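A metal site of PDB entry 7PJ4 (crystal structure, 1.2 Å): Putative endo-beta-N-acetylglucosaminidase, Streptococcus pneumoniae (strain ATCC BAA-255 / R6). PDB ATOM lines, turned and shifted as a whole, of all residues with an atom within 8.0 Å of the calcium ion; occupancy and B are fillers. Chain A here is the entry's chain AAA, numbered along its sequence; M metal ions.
OD1 of Asp 16 is in hydrogen-bond range of N of Gly 19, 3.2 Å away.
Of the 8 residues printed, 3 come within 4 Å of the calcium ion.
The nearest printed residue that does not touch the calcium ion is Ser 17 (6.1 Å).
OE1 of Glu 20 binds the calcium ion (2.2 Å).
The calcium ion is bound by OD2 of Asp 16 (2.4 Å).
OD2 of Asp 18 binds the calcium ion.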
ATOM      1  N   TYR A  15       3.055 -14.951  10.778  1.00  0.00           N
ATOM      2  CA  TYR A  15       1.902 -15.728  11.237  1.00  0.00           C
ATOM      3  C   TYR A  15       2.281 -16.654  12.375  1.00  0.00           C
ATOM      4  O   TYR A  15       3.442 -17.042  12.533  1.00  0.00           O
ATOM      5  CB  TYR A  15       1.396 -16.578  10.058  1.00  0.00           C
ATOM      6  CG  TYR A  15       0.969 -15.802   8.844  1.00  0.00           C
ATOM      7  CD1 TYR A  15      -0.331 -15.365   8.669  1.00  0.00           C
ATOM      8  CD2 TYR A  15       1.882 -15.527   7.836  1.00  0.00           C
ATOM      9  CE1 TYR A  15      -0.713 -14.658   7.544  1.00  0.00           C
ATOM     10  CE2 TYR A  15       1.518 -14.827   6.696  1.00  0.00           C
ATOM     11  CZ  TYR A  15       0.209 -14.410   6.541  1.00  0.00           C
ATOM     12  OH  TYR A  15      -0.147 -13.717   5.429  1.00  0.00           O
ATOM     13  N   ASP A  16       1.280 -17.056  13.142  1.00  0.00           N
ATOM     14  CA  ASP A  16       1.458 -18.112  14.147  1.00  0.00           C
ATOM     15  C   ASP A  16       1.184 -19.479  13.509  1.00  0.00           C
ATOM     16  O   ASP A  16       0.876 -19.581  12.301  1.00  0.00           O
ATOM     17  CB  ASP A  16       0.624 -17.858  15.405  1.00  0.00           C
ATOM     18  CG  ASP A  16      -0.867 -18.118  15.333  1.00  0.00           C
ATOM     19  OD1 ASP A  16      -1.338 -18.527  14.272  1.00  0.00           O
ATOM     20  OD2 ASP A  16      -1.539 -17.835  16.363  1.00  0.00           O
ATOM     21  N   SER A  17       1.219 -20.541  14.313  1.00  0.00           N
ATOM     22  CA  SER A  17       1.029 -21.912  13.774  1.00  0.00           C
ATOM     23  C   SER A  17      -0.415 -22.168  13.328  1.00  0.00           C
ATOM     24  O   SER A  17      -0.594 -23.142  12.585  1.00  0.00           O
ATOM     25  CB  SER A  17       1.484 -22.920  14.786  1.00  0.00           C
ATOM     26  OG  SER A  17       0.773 -22.767  15.983  1.00  0.00           O
ATOM     27  N   ASP A  18      -1.377 -21.341  13.755  1.00  0.00           N
ATOM     28  CA  ASP A  18      -2.808 -21.418  13.366  1.00  0.00           C
ATOM     29  C   ASP A  18      -3.027 -20.660  12.054  1.00  0.00           C
ATOM     30  O   ASP A  18      -4.151 -20.656  11.551  1.00  0.00           O
ATOM     31  CB  ASP A  18      -3.746 -20.822  14.426  1.00  0.00           C
ATOM     32  CG  ASP A  18      -3.620 -21.445  15.806  1.00  0.00           C
ATOM     33  OD1 ASP A  18      -3.543 -22.667  15.856  1.00  0.00           O
ATOM     34  OD2 ASP A  18      -3.617 -20.669  16.806  1.00  0.00           O
ATOM     35  N   GLY A  19      -2.004 -19.976  11.521  1.00  0.00           N
ATOM     36  CA  GLY A  19      -2.222 -19.122  10.357  1.00  0.00           C
ATOM     37  C   GLY A  19      -2.749 -17.739  10.716  1.00  0.00           C
ATOM     38  O   GLY A  19      -3.118 -17.012   9.803  1.00  0.00           O
ATOM     39  N   GLU A  20      -2.775 -17.366  11.998  1.00  0.00           N
ATOM     40  CA  GLU A  20      -3.251 -16.011  12.368  1.00  0.00           C
ATOM     41  C   GLU A  20      -2.086 -15.041  12.228  1.00  0.00           C
ATOM     42  O   GLU A  20      -0.929 -15.391  12.502  1.00  0.00           O
ATOM     43  CB  GLU A  20      -3.858 -15.987  13.757  1.00  0.00           C
ATOM     44  CG  GLU A  20      -5.112 -16.816  13.847  1.00  0.00           C
ATOM     45  CD  GLU A  20      -5.642 -16.891  15.264  1.00  0.00           C
ATOM     46  OE1 GLU A  20      -5.001 -17.586  16.085  1.00  0.00           O
ATOM     47  OE2 GLU A  20      -6.656 -16.231  15.533  1.00  0.00           O
ATOM     48  N   LYS A  21      -2.404 -13.827  11.815  1.00  0.00           N
ATOM     49  CA  LYS A  21      -1.383 -12.780  11.670  1.00  0.00           C
ATOM     50  C   LYS A  21      -0.933 -12.306  13.053  1.00  0.00           C
ATOM     51  O   LYS A  21      -1.769 -11.936  13.876  1.00  0.00           O
ATOM     52  CB  LYS A  21      -1.961 -11.618  10.869  1.00  0.00           C
ATOM     53  CG  LYS A  21      -2.334 -11.966   9.442  1.00  0.00           C
ATOM     54  CD  LYS A  21      -2.972 -10.815   8.738  1.00  0.00           C
ATOM     55  CE  LYS A  21      -3.727 -11.220   7.506  1.00  0.00           C
ATOM     56  NZ  LYS A  21      -4.666 -10.153   7.101  1.00  0.00           N
ATOM     57  N   LEU A  22       0.377 -12.318  13.285  1.00  0.00           N
ATOM     58  CA  LEU A  22       0.984 -11.757  14.516  1.00  0.00           C
ATOM     59  C   LEU A  22       1.453 -10.328  14.298  1.00  0.00           C
ATOM     60  O   LEU A  22       1.392  -9.518  15.224  1.00  0.00           O
ATOM     61  CB  LEU A  22       2.134 -12.640  14.945  1.00  0.00           C
ATOM     62  CG  LEU A  22       1.722 -14.050  15.336  1.00  0.00           C
ATOM     63  CD1 LEU A  22       2.958 -14.887  15.640  1.00  0.00           C
ATOM     64  CD2 LEU A  22       0.753 -14.032  16.490  1.00  0.00           C
HETATM   65 CA    CA M   1      -3.521 -18.337  17.549  1.00  0.00          CA
